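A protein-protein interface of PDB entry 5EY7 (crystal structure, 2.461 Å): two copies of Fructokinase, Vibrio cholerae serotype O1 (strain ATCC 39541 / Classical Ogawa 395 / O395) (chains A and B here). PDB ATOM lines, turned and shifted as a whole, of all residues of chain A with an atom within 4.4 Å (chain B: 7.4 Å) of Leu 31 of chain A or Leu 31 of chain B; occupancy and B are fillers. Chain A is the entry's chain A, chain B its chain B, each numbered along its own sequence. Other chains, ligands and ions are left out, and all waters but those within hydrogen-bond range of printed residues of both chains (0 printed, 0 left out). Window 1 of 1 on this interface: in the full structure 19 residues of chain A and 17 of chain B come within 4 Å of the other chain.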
ATOM      1  N   VAL A  29     -17.140  10.908   0.537  1.00  0.00           N
ATOM      2  CA  VAL A  29     -17.603  12.265   0.781  1.00  0.00           C
ATOM      3  C   VAL A  29     -18.110  12.863  -0.529  1.00  0.00           C
ATOM      4  O   VAL A  29     -17.357  12.999  -1.494  1.00  0.00           O
ATOM      5  CB  VAL A  29     -16.492  13.153   1.371  1.00  0.00           C
ATOM      6  CG1 VAL A  29     -16.953  14.601   1.446  1.00  0.00           C
ATOM      7  CG2 VAL A  29     -16.089  12.646   2.750  1.00  0.00           C
ATOM      8  N   ASP A  30     -19.396  13.194  -0.562  1.00  0.00           N
ATOM      9  CA  ASP A  30     -20.017  13.774  -1.747  1.00  0.00           C
ATOM     10  C   ASP A  30     -20.039  15.295  -1.670  1.00  0.00           C
ATOM     11  O   ASP A  30     -20.459  15.866  -0.664  1.00  0.00           O
ATOM     12  CB  ASP A  30     -21.444  13.249  -1.921  1.00  0.00           C
ATOM     13  CG  ASP A  30     -21.484  11.782  -2.290  1.00  0.00           C
ATOM     14  OD1 ASP A  30     -20.406  11.151  -2.342  1.00  0.00           O
ATOM     15  OD2 ASP A  30     -22.597  11.259  -2.519  1.00  0.00           O
ATOM     16  N   LEU A  31     -19.589  15.941  -2.740  1.00  0.00           N
ATOM     17  CA  LEU A  31     -19.636  17.393  -2.838  1.00  0.00           C
ATOM     18  C   LEU A  31     -20.770  17.807  -3.764  1.00  0.00           C
ATOM     19  O   LEU A  31     -20.660  17.695  -4.985  1.00  0.00           O
ATOM     20  CB  LEU A  31     -18.303  17.939  -3.339  1.00  0.00           C
ATOM     21  CG  LEU A  31     -17.092  17.562  -2.485  1.00  0.00           C
ATOM     22  CD1 LEU A  31     -15.791  17.950  -3.175  1.00  0.00           C
ATOM     23  CD2 LEU A  31     -17.189  18.202  -1.110  1.00  0.00           C
ATOM     24  N   ILE A  32     -21.862  18.282  -3.175  1.00  0.00           N
ATOM     25  CA  ILE A  32     -23.069  18.582  -3.931  1.00  0.00           C
ATOM     26  C   ILE A  32     -23.282  20.088  -4.066  1.00  0.00           C
ATOM     27  O   ILE A  32     -23.193  20.820  -3.079  1.00  0.00           O
ATOM     28  CB  ILE A  32     -24.308  17.927  -3.276  1.00  0.00           C
ATOM     29  CG1 ILE A  32     -23.964  16.513  -2.794  1.00  0.00           C
ATOM     30  CG2 ILE A  32     -25.482  17.894  -4.245  1.00  0.00           C
ATOM     31  CD1 ILE A  32     -25.163  15.648  -2.468  1.00  0.00           C
ATOM     32  N   PRO A  33     -23.558  20.551  -5.303  1.00  0.00           N
ATOM     33  CA  PRO A  33     -23.668  21.984  -5.598  1.00  0.00           C
ATOM     34  C   PRO A  33     -24.729  22.697  -4.778  1.00  0.00           C
ATOM     35  O   PRO A  33     -25.901  22.325  -4.814  1.00  0.00           O
ATOM     36  CB  PRO A  33     -24.047  22.009  -7.086  1.00  0.00           C
ATOM     37  CG  PRO A  33     -23.510  20.742  -7.623  1.00  0.00           C
ATOM     38  CD  PRO A  33     -23.711  19.744  -6.527  1.00  0.00           C
ATOM     39  N   TYR A  39     -20.252  24.115  -2.365  1.00  0.00           N
ATOM     40  CA  TYR A  39     -20.522  22.684  -2.368  1.00  0.00           C
ATOM     41  C   TYR A  39     -20.980  22.201  -1.000  1.00  0.00           C
ATOM     42  O   TYR A  39     -20.459  22.631   0.025  1.00  0.00           O
ATOM     43  CB  TYR A  39     -19.280  21.901  -2.805  1.00  0.00           C
ATOM     44  CG  TYR A  39     -19.160  21.715  -4.299  1.00  0.00           C
ATOM     45  CD1 TYR A  39     -20.236  21.266  -5.049  1.00  0.00           C
ATOM     46  CD2 TYR A  39     -17.978  22.000  -4.959  1.00  0.00           C
ATOM     47  CE1 TYR A  39     -20.135  21.096  -6.416  1.00  0.00           C
ATOM     48  CE2 TYR A  39     -17.864  21.835  -6.325  1.00  0.00           C
ATOM     49  CZ  TYR A  39     -18.945  21.384  -7.049  1.00  0.00           C
ATOM     50  OH  TYR A  39     -18.838  21.220  -8.410  1.00  0.00           O
ATOM     51  N   LEU A  40     -21.961  21.308  -0.997  1.00  0.00           N
ATOM     52  CA  LEU A  40     -22.406  20.666   0.229  1.00  0.00           C
ATOM     53  C   LEU A  40     -21.496  19.495   0.577  1.00  0.00           C
ATOM     54  O   LEU A  40     -21.314  18.581  -0.228  1.00  0.00           O
ATOM     55  CB  LEU A  40     -23.851  20.184   0.091  1.00  0.00           C
ATOM     56  CG  LEU A  40     -24.967  21.148   0.491  1.00  0.00           C
ATOM     57  CD1 LEU A  40     -26.328  20.532   0.201  1.00  0.00           C
ATOM     58  CD2 LEU A  40     -24.846  21.502   1.961  1.00  0.00           C
ATOM     59  N   THR A 100     -13.522  10.736  -2.983  1.00  0.00           N
ATOM     60  CA  THR A 100     -14.273  11.982  -3.090  1.00  0.00           C
ATOM     61  C   THR A 100     -15.017  12.054  -4.419  1.00  0.00           C
ATOM     62  O   THR A 100     -14.408  11.983  -5.483  1.00  0.00           O
ATOM     63  CB  THR A 100     -13.362  13.219  -2.965  1.00  0.00           C
ATOM     64  OG1 THR A 100     -12.616  13.156  -1.742  1.00  0.00           O
ATOM     65  CG2 THR A 100     -14.196  14.490  -2.983  1.00  0.00           C
ATOM     66  N   VAL A 101     -16.336  12.195  -4.351  1.00  0.00           N
ATOM     67  CA  VAL A 101     -17.159  12.304  -5.552  1.00  0.00           C
ATOM     68  C   VAL A 101     -17.771  13.693  -5.682  1.00  0.00           C
ATOM     69  O   VAL A 101     -18.387  14.198  -4.746  1.00  0.00           O
ATOM     70  CB  VAL A 101     -18.292  11.256  -5.565  1.00  0.00           C
ATOM     71  CG1 VAL A 101     -19.355  11.629  -6.593  1.00  0.00           C
ATOM     72  CG2 VAL A 101     -17.730   9.870  -5.853  1.00  0.00           C
ATOM     73  N   VAL A 102     -17.585  14.309  -6.845  1.00  0.00           N
ATOM     74  CA  VAL A 102     -18.190  15.599  -7.138  1.00  0.00           C
ATOM     75  C   VAL A 102     -19.380  15.416  -8.060  1.00  0.00           C
ATOM     76  O   VAL A 102     -19.224  15.061  -9.226  1.00  0.00           O
ATOM     77  CB  VAL A 102     -17.193  16.571  -7.799  1.00  0.00           C
ATOM     78  CG1 VAL A 102     -17.902  17.860  -8.214  1.00  0.00           C
ATOM     79  CG2 VAL A 102     -16.041  16.870  -6.857  1.00  0.00           C
ATOM     80  N   VAL A 103     -20.572  15.649  -7.532  1.00  0.00           N
ATOM     81  CA  VAL A 103     -21.770  15.572  -8.345  1.00  0.00           C
ATOM     82  C   VAL A 103     -22.029  16.927  -8.985  1.00  0.00           C
ATOM     83  O   VAL A 103     -21.985  17.962  -8.328  1.00  0.00           O
ATOM     84  CB  VAL A 103     -22.996  15.118  -7.522  1.00  0.00           C
ATOM     85  CG1 VAL A 103     -22.953  15.709  -6.135  1.00  0.00           C
ATOM     86  CG2 VAL A 103     -24.295  15.479  -8.236  1.00  0.00           C
ATOM     87  N   VAL B  28      -5.534  24.817 -10.066  1.00  0.00           N
ATOM     88  CA  VAL B  28      -5.987  24.184  -8.832  1.00  0.00           C
ATOM     89  C   VAL B  28      -7.258  24.796  -8.250  1.00  0.00           C
ATOM     90  O   VAL B  28      -7.383  26.013  -8.147  1.00  0.00           O
ATOM     91  CB  VAL B  28      -4.883  24.241  -7.761  1.00  0.00           C
ATOM     92  CG1 VAL B  28      -5.356  23.585  -6.476  1.00  0.00           C
ATOM     93  CG2 VAL B  28      -3.620  23.565  -8.269  1.00  0.00           C
ATOM     94  N   VAL B  29      -8.201  23.938  -7.871  1.00  0.00           N
ATOM     95  CA  VAL B  29      -9.401  24.380  -7.176  1.00  0.00           C
ATOM     96  C   VAL B  29      -9.234  24.196  -5.672  1.00  0.00           C
ATOM     97  O   VAL B  29      -9.028  23.081  -5.196  1.00  0.00           O
ATOM     98  CB  VAL B  29     -10.649  23.614  -7.653  1.00  0.00           C
ATOM     99  CG1 VAL B  29     -11.830  23.867  -6.721  1.00  0.00           C
ATOM    100  CG2 VAL B  29     -10.993  23.997  -9.086  1.00  0.00           C
ATOM    101  N   ASP B  30      -9.304  25.298  -4.934  1.00  0.00           N
ATOM    102  CA  ASP B  30      -9.223  25.259  -3.477  1.00  0.00           C
ATOM    103  C   ASP B  30     -10.613  25.182  -2.849  1.00  0.00           C
ATOM    104  O   ASP B  30     -11.502  25.961  -3.195  1.00  0.00           O
ATOM    105  CB  ASP B  30      -8.483  26.489  -2.939  1.00  0.00           C
ATOM    106  CG  ASP B  30      -6.982  26.407  -3.137  1.00  0.00           C
ATOM    107  OD1 ASP B  30      -6.421  25.303  -3.003  1.00  0.00           O
ATOM    108  OD2 ASP B  30      -6.358  27.450  -3.417  1.00  0.00           O
ATOM    109  N   LEU B  31     -10.793  24.235  -1.931  1.00  0.00           N
ATOM    110  CA  LEU B  31     -12.054  24.089  -1.211  1.00  0.00           C
ATOM    111  C   LEU B  31     -11.933  24.589   0.229  1.00  0.00           C
ATOM    112  O   LEU B  31     -11.288  23.958   1.063  1.00  0.00           O
ATOM    113  CB  LEU B  31     -12.509  22.629  -1.229  1.00  0.00           C
ATOM    114  CG  LEU B  31     -12.872  22.086  -2.613  1.00  0.00           C
ATOM    115  CD1 LEU B  31     -13.318  20.635  -2.531  1.00  0.00           C
ATOM    116  CD2 LEU B  31     -13.948  22.945  -3.257  1.00  0.00           C
ATOM    117  N   ILE B  32     -12.552  25.730   0.516  1.00  0.00           N
ATOM    118  CA  ILE B  32     -12.437  26.360   1.829  1.00  0.00           C
ATOM    119  C   ILE B  32     -13.695  26.154   2.672  1.00  0.00           C
ATOM    120  O   ILE B  32     -14.808  26.318   2.175  1.00  0.00           O
ATOM    121  CB  ILE B  32     -12.158  27.877   1.704  1.00  0.00           C
ATOM    122  CG1 ILE B  32     -11.139  28.156   0.595  1.00  0.00           C
ATOM    123  CG2 ILE B  32     -11.667  28.440   3.028  1.00  0.00           C
ATOM    124  CD1 ILE B  32      -9.738  27.660   0.907  1.00  0.00           C
ATOM    125  N   PRO B  33     -13.518  25.776   3.954  1.00  0.00           N
ATOM    126  CA  PRO B  33     -14.662  25.603   4.854  1.00  0.00           C
ATOM    127  C   PRO B  33     -15.462  26.878   5.020  1.00  0.00           C
ATOM    128  O   PRO B  33     -14.967  27.847   5.595  1.00  0.00           O
ATOM    129  CB  PRO B  33     -14.007  25.205   6.181  1.00  0.00           C
ATOM    130  CG  PRO B  33     -12.746  24.552   5.779  1.00  0.00           C
ATOM    131  CD  PRO B  33     -12.268  25.325   4.588  1.00  0.00           C
ATOM    132  N   ASP B  34     -16.687  26.874   4.508  1.00  0.00           N
ATOM    133  CA  ASP B  34     -17.573  28.023   4.629  1.00  0.00           C
ATOM    134  C   ASP B  34     -18.449  27.877   5.865  1.00  0.00           C
ATOM    135  O   ASP B  34     -19.672  27.973   5.791  1.00  0.00           O
ATOM    136  CB  ASP B  34     -18.439  28.171   3.377  1.00  0.00           C
ATOM    137  CG  ASP B  34     -19.188  29.485   3.343  1.00  0.00           C
ATOM    138  OD1 ASP B  34     -18.525  30.535   3.223  1.00  0.00           O
ATOM    139  OD2 ASP B  34     -20.434  29.467   3.438  1.00  0.00           O
ATOM    140  N   HIS B  38     -20.338  23.112   4.405  1.00  0.00           N
ATOM    141  CA  HIS B  38     -20.252  23.869   3.161  1.00  0.00           C
ATOM    142  C   HIS B  38     -18.806  24.192   2.807  1.00  0.00           C
ATOM    143  O   HIS B  38     -18.038  24.649   3.650  1.00  0.00           O
ATOM    144  CB  HIS B  38     -21.069  25.164   3.254  1.00  0.00           C
ATOM    145  CG  HIS B  38     -22.466  25.039   2.744  1.00  0.00           C
ATOM    146  ND1 HIS B  38     -23.568  24.969   3.577  1.00  0.00           N
ATOM    147  CD2 HIS B  38     -22.957  24.985   1.479  1.00  0.00           C
ATOM    148  CE1 HIS B  38     -24.663  24.874   2.848  1.00  0.00           C
ATOM    149  NE2 HIS B  38     -24.323  24.879   1.577  1.00  0.00           N
ATOM    150  N   TYR B  39     -18.440  23.944   1.556  1.00  0.00           N
ATOM    151  CA  TYR B  39     -17.140  24.359   1.050  1.00  0.00           C
ATOM    152  C   TYR B  39     -17.308  25.474   0.033  1.00  0.00           C
ATOM    153  O   TYR B  39     -18.258  25.478  -0.746  1.00  0.00           O
ATOM    154  CB  TYR B  39     -16.393  23.187   0.413  1.00  0.00           C
ATOM    155  CG  TYR B  39     -15.680  22.281   1.391  1.00  0.00           C
ATOM    156  CD1 TYR B  39     -14.555  22.714   2.074  1.00  0.00           C
ATOM    157  CD2 TYR B  39     -16.120  20.985   1.611  1.00  0.00           C
ATOM    158  CE1 TYR B  39     -13.896  21.884   2.962  1.00  0.00           C
ATOM    159  CE2 TYR B  39     -15.465  20.145   2.495  1.00  0.00           C
ATOM    160  CZ  TYR B  39     -14.356  20.601   3.168  1.00  0.00           C
ATOM    161  OH  TYR B  39     -13.702  19.775   4.049  1.00  0.00           O
ATOM    162  N   LEU B  40     -16.390  26.430   0.056  1.00  0.00           N
ATOM    163  CA  LEU B  40     -16.375  27.492  -0.941  1.00  0.00           C
ATOM    164  C   LEU B  40     -15.418  27.128  -2.068  1.00  0.00           C
ATOM    165  O   LEU B  40     -14.292  26.700  -1.820  1.00  0.00           O
ATOM    166  CB  LEU B  40     -15.970  28.827  -0.312  1.00  0.00           C
ATOM    167  CG  LEU B  40     -15.633  29.988  -1.253  1.00  0.00           C
ATOM    168  CD1 LEU B  40     -16.825  30.352  -2.124  1.00  0.00           C
ATOM    169  CD2 LEU B  40     -15.159  31.196  -0.459  1.00  0.00           C
ATOM    170  N   LYS B  41     -15.872  27.284  -3.307  1.00  0.00           N
ATOM    171  CA  LYS B  41     -15.015  27.046  -4.465  1.00  0.00           C
ATOM    172  C   LYS B  41     -14.148  28.266  -4.752  1.00  0.00           C
ATOM    173  O   LYS B  41     -14.659  29.349  -5.035  1.00  0.00           O
ATOM    174  CB  LYS B  41     -15.840  26.697  -5.700  1.00  0.00           C
ATOM    175  CG  LYS B  41     -16.172  25.223  -5.816  1.00  0.00           C
ATOM    176  CD  LYS B  41     -16.510  24.842  -7.243  1.00  0.00           C
ATOM    177  CE  LYS B  41     -17.867  25.377  -7.666  1.00  0.00           C
ATOM    178  NZ  LYS B  41     -18.245  24.861  -9.010  1.00  0.00           N
ATOM    179  N   CYS B  42     -12.835  28.082  -4.670  1.00  0.00           N
ATOM    180  CA  CYS B  42     -11.884  29.154  -4.936  1.00  0.00           C
ATOM    181  C   CYS B  42     -10.817  28.727  -5.934  1.00  0.00           C
ATOM    182  O   CYS B  42     -10.068  27.786  -5.684  1.00  0.00           O
ATOM    183  CB  CYS B  42     -11.231  29.624  -3.633  1.00  0.00           C
ATOM    184  SG  CYS B  42     -12.291  30.662  -2.601  1.00  0.00           S
ATOM    185  N   PRO B  43     -10.748  29.430  -7.080  1.00  0.00           N
ATOM    186  CA  PRO B  43      -9.738  29.128  -8.102  1.00  0.00           C
ATOM    187  C   PRO B  43      -8.329  29.442  -7.622  1.00  0.00           C
ATOM    188  O   PRO B  43      -8.099  30.496  -7.043  1.00  0.00           O
ATOM    189  CB  PRO B  43     -10.130  30.046  -9.268  1.00  0.00           C
ATOM    190  CG  PRO B  43     -10.853  31.182  -8.613  1.00  0.00           C
ATOM    191  CD  PRO B  43     -11.603  30.567  -7.473  1.00  0.00           C
ATOM    192  N   PHE B  72     -14.325  20.507 -11.743  1.00  0.00           N
ATOM    193  CA  PHE B  72     -13.262  21.380 -11.244  1.00  0.00           C
ATOM    194  C   PHE B  72     -12.402  21.932 -12.381  1.00  0.00           C
ATOM    195  O   PHE B  72     -11.973  23.084 -12.345  1.00  0.00           O
ATOM    196  CB  PHE B  72     -12.382  20.643 -10.229  1.00  0.00           C
ATOM    197  CG  PHE B  72     -13.044  20.432  -8.907  1.00  0.00           C
ATOM    198  CD1 PHE B  72     -14.191  21.132  -8.584  1.00  0.00           C
ATOM    199  CD2 PHE B  72     -12.528  19.537  -7.988  1.00  0.00           C
ATOM    200  CE1 PHE B  72     -14.814  20.947  -7.370  1.00  0.00           C
ATOM    201  CE2 PHE B  72     -13.148  19.344  -6.763  1.00  0.00           C
ATOM    202  CZ  PHE B  72     -14.294  20.054  -6.455  1.00  0.00           C
ATOM    203  N   THR B 100      -6.903  19.230  -6.675  1.00  0.00           N
ATOM    204  CA  THR B 100      -7.898  19.715  -5.729  1.00  0.00           C
ATOM    205  C   THR B 100      -7.361  19.757  -4.301  1.00  0.00           C
ATOM    206  O   THR B 100      -6.912  18.748  -3.764  1.00  0.00           O
ATOM    207  CB  THR B 100      -9.159  18.840  -5.762  1.00  0.00           C
ATOM    208  OG1 THR B 100      -9.660  18.779  -7.103  1.00  0.00           O
ATOM    209  CG2 THR B 100     -10.230  19.413  -4.844  1.00  0.00           C
ATOM    210  N   VAL B 101      -7.417  20.933  -3.690  1.00  0.00           N
ATOM    211  CA  VAL B 101      -6.946  21.098  -2.321  1.00  0.00           C
ATOM    212  C   VAL B 101      -8.100  21.340  -1.355  1.00  0.00           C
ATOM    213  O   VAL B 101      -9.019  22.105  -1.642  1.00  0.00           O
ATOM    214  CB  VAL B 101      -5.947  22.264  -2.200  1.00  0.00           C
ATOM    215  CG1 VAL B 101      -5.360  22.314  -0.798  1.00  0.00           C
ATOM    216  CG2 VAL B 101      -4.840  22.125  -3.224  1.00  0.00           C
ATOM    217  N   VAL B 102      -8.043  20.670  -0.209  1.00  0.00           N
ATOM    218  CA  VAL B 102      -9.002  20.886   0.863  1.00  0.00           C
ATOM    219  C   VAL B 102      -8.263  21.368   2.103  1.00  0.00           C
ATOM    220  O   VAL B 102      -7.403  20.663   2.625  1.00  0.00           O
ATOM    221  CB  VAL B 102      -9.781  19.601   1.197  1.00  0.00           C
ATOM    222  CG1 VAL B 102     -10.731  19.838   2.368  1.00  0.00           C
ATOM    223  CG2 VAL B 102     -10.539  19.105  -0.027  1.00  0.00           C
ATOM    224  N   VAL B 103      -8.581  22.573   2.565  1.00  0.00           N
ATOM    225  CA  VAL B 103      -7.945  23.097   3.767  1.00  0.00           C
ATOM    226  C   VAL B 103      -8.789  22.751   4.993  1.00  0.00           C
ATOM    227  O   VAL B 103     -10.016  22.720   4.931  1.00  0.00           O
ATOM    228  CB  VAL B 103      -7.711  24.629   3.683  1.00  0.00           C
ATOM    229  CG1 VAL B 103      -6.903  24.979   2.448  1.00  0.00           C
ATOM    230  CG2 VAL B 103      -9.012  25.377   3.669  1.00  0.00           C
ATOM    231  N   ASP B 104      -8.115  22.471   6.102  1.00  0.00           N
ATOM    232  CA  ASP B 104      -8.771  21.948   7.294  1.00  0.00           C
ATOM    233  C   ASP B 104      -8.423  22.779   8.528  1.00  0.00           C
ATOM    234  O   ASP B 104      -7.379  23.429   8.573  1.00  0.00           O
ATOM    235  CB  ASP B 104      -8.377  20.484   7.506  1.00  0.00           C
ATOM    236  CG  ASP B 104      -9.251  19.784   8.526  1.00  0.00           C
ATOM    237  OD1 ASP B 104     -10.430  19.516   8.212  1.00  0.00           O
ATOM    238  OD2 ASP B 104      -8.755  19.492   9.634  1.00  0.00           O
ATOM    239  N   MET B 116      -5.688  16.396  -2.572  1.00  0.00           N
ATOM    240  CA  MET B 116      -6.665  15.326  -2.696  1.00  0.00           C
ATOM    241  C   MET B 116      -6.361  14.388  -3.855  1.00  0.00           C
ATOM    242  O   MET B 116      -6.683  13.200  -3.800  1.00  0.00           O
ATOM    243  CB  MET B 116      -8.058  15.916  -2.866  1.00  0.00           C
ATOM    244  CG  MET B 116      -9.169  14.904  -2.718  1.00  0.00           C
ATOM    245  SD  MET B 116     -10.781  15.690  -2.743  1.00  0.00           S
ATOM    246  CE  MET B 116     -11.015  15.930  -4.497  1.00  0.00           C
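N of Leu 31 of chain A lies within hydrogen-bond range of O of Val 101 of chain A (2.9 Å).
O of Thr 100 of chain B is in hydrogen-bond range of N of Met 116 of chain B (2.9 Å).
The backbone NH of Leu 31 of chain B is in hydrogen-bond range of the backbone carbonyl oxygen of Val 101 of chain B (2.8 Å).
The backbone carbonyl oxygen of Leu 31 of chain B is in hydrogen-bond range of the backbone NH of Val 103 of chain B, at 3.4 Å.
The backbone NH of Val 103 of chain A lies close to the backbone carbonyl oxygen of Leu 31 of chain A, at 3.3 Å.
The backbone carbonyl oxygen (O) of Ile 32 of chain A lies within hydrogen-bond range of the backbone NH (N) of Leu 40 of chain A, at 2.5 Å.
CD1 of Leu 31 of chain B touches CD1 of Leu 31 of chain A, at 3.7 Å.
Tyr 39 of chain A touches His 38 of chain B (O to CA, 3.4 Å).
CE2 of Tyr 39 of chain A touches CD of Lys 41 of chain B, 3.4 Å away.
Phe 72 of chain B touches Tyr 39 of chain A.
His 38 of chain B touches Leu 40 of chain A (NE2 to CD2, 3.4 Å).
CG2 of Val 102 of chain A touches CZ of Phe 72 of chain B, at 3.7 Å.
Of the 20 printed residues of chain B, 6 touch a printed residue of chain A.
Hydrophobic or aromatic side chains of chain B that line the printed part of chain A: Leu 31, His 38, Phe 72 and Met 116.
Of the 11 printed residues of chain A, 5 touch a printed residue of chain B.
Printed residues of chain A that touch a printed residue of chain B: Leu 31, Tyr 39, Leu 40, Thr 100 and Val 102.
Of the printed residues of chain B, Leu 31 of chain A touches Leu 31 (3.7 Å).
Printed residues of chain A within 4 Å of Leu 31 of chain B: Leu 31 (3.7 Å).
Printed residues of chain B within 4 Å of Thr 100 of chain A: Met 116 (3.3 Å).
Of the printed residues of chain A, Met 116 of chain B touches Thr 100 (3.3 Å).
Printed residues of chain A within 4 Å of Lys 41 of chain B: Tyr 39 (3.4 Å).
Thr 100 of chain B touches none of the printed residues of chain A.
Val 101 of chain B touches none of the printed residues of chain A.
The nearest residue of chain B that does not touch Leu 31 of chain A is Tyr 39 of chain B (4.04 Å).
The nearest printed residue of chain A that does not touch Leu 31 of chain B is Tyr 39 of chain A (4.5 Å).
The nearest printed residue of chain A that does not touch Met 116 of chain B is Leu 31 of chain A (5.4 Å).
Leu 31 of chain B touches its own counterpart, Leu 31 of chain A.
Tyr 39 of chain B touches its own counterpart, Tyr 39 of chain A.
Positions printed for both chains: 29, 30, 31, 32, 33, 39, 40, 100, 101, 102 and 103.
Of the 8 pairs that touch across the chains among the printed residues, 2 have their exchanged pair printed and touching as well.
OG1 of Thr 100 of chain A sits at hydrogen-bond distance from SD of Met 116 of chain B, 3.3 Å away.
N of Tyr 39 of chain B sits at hydrogen-bond distance from O of Tyr 39 of chain A (2.9 Å).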
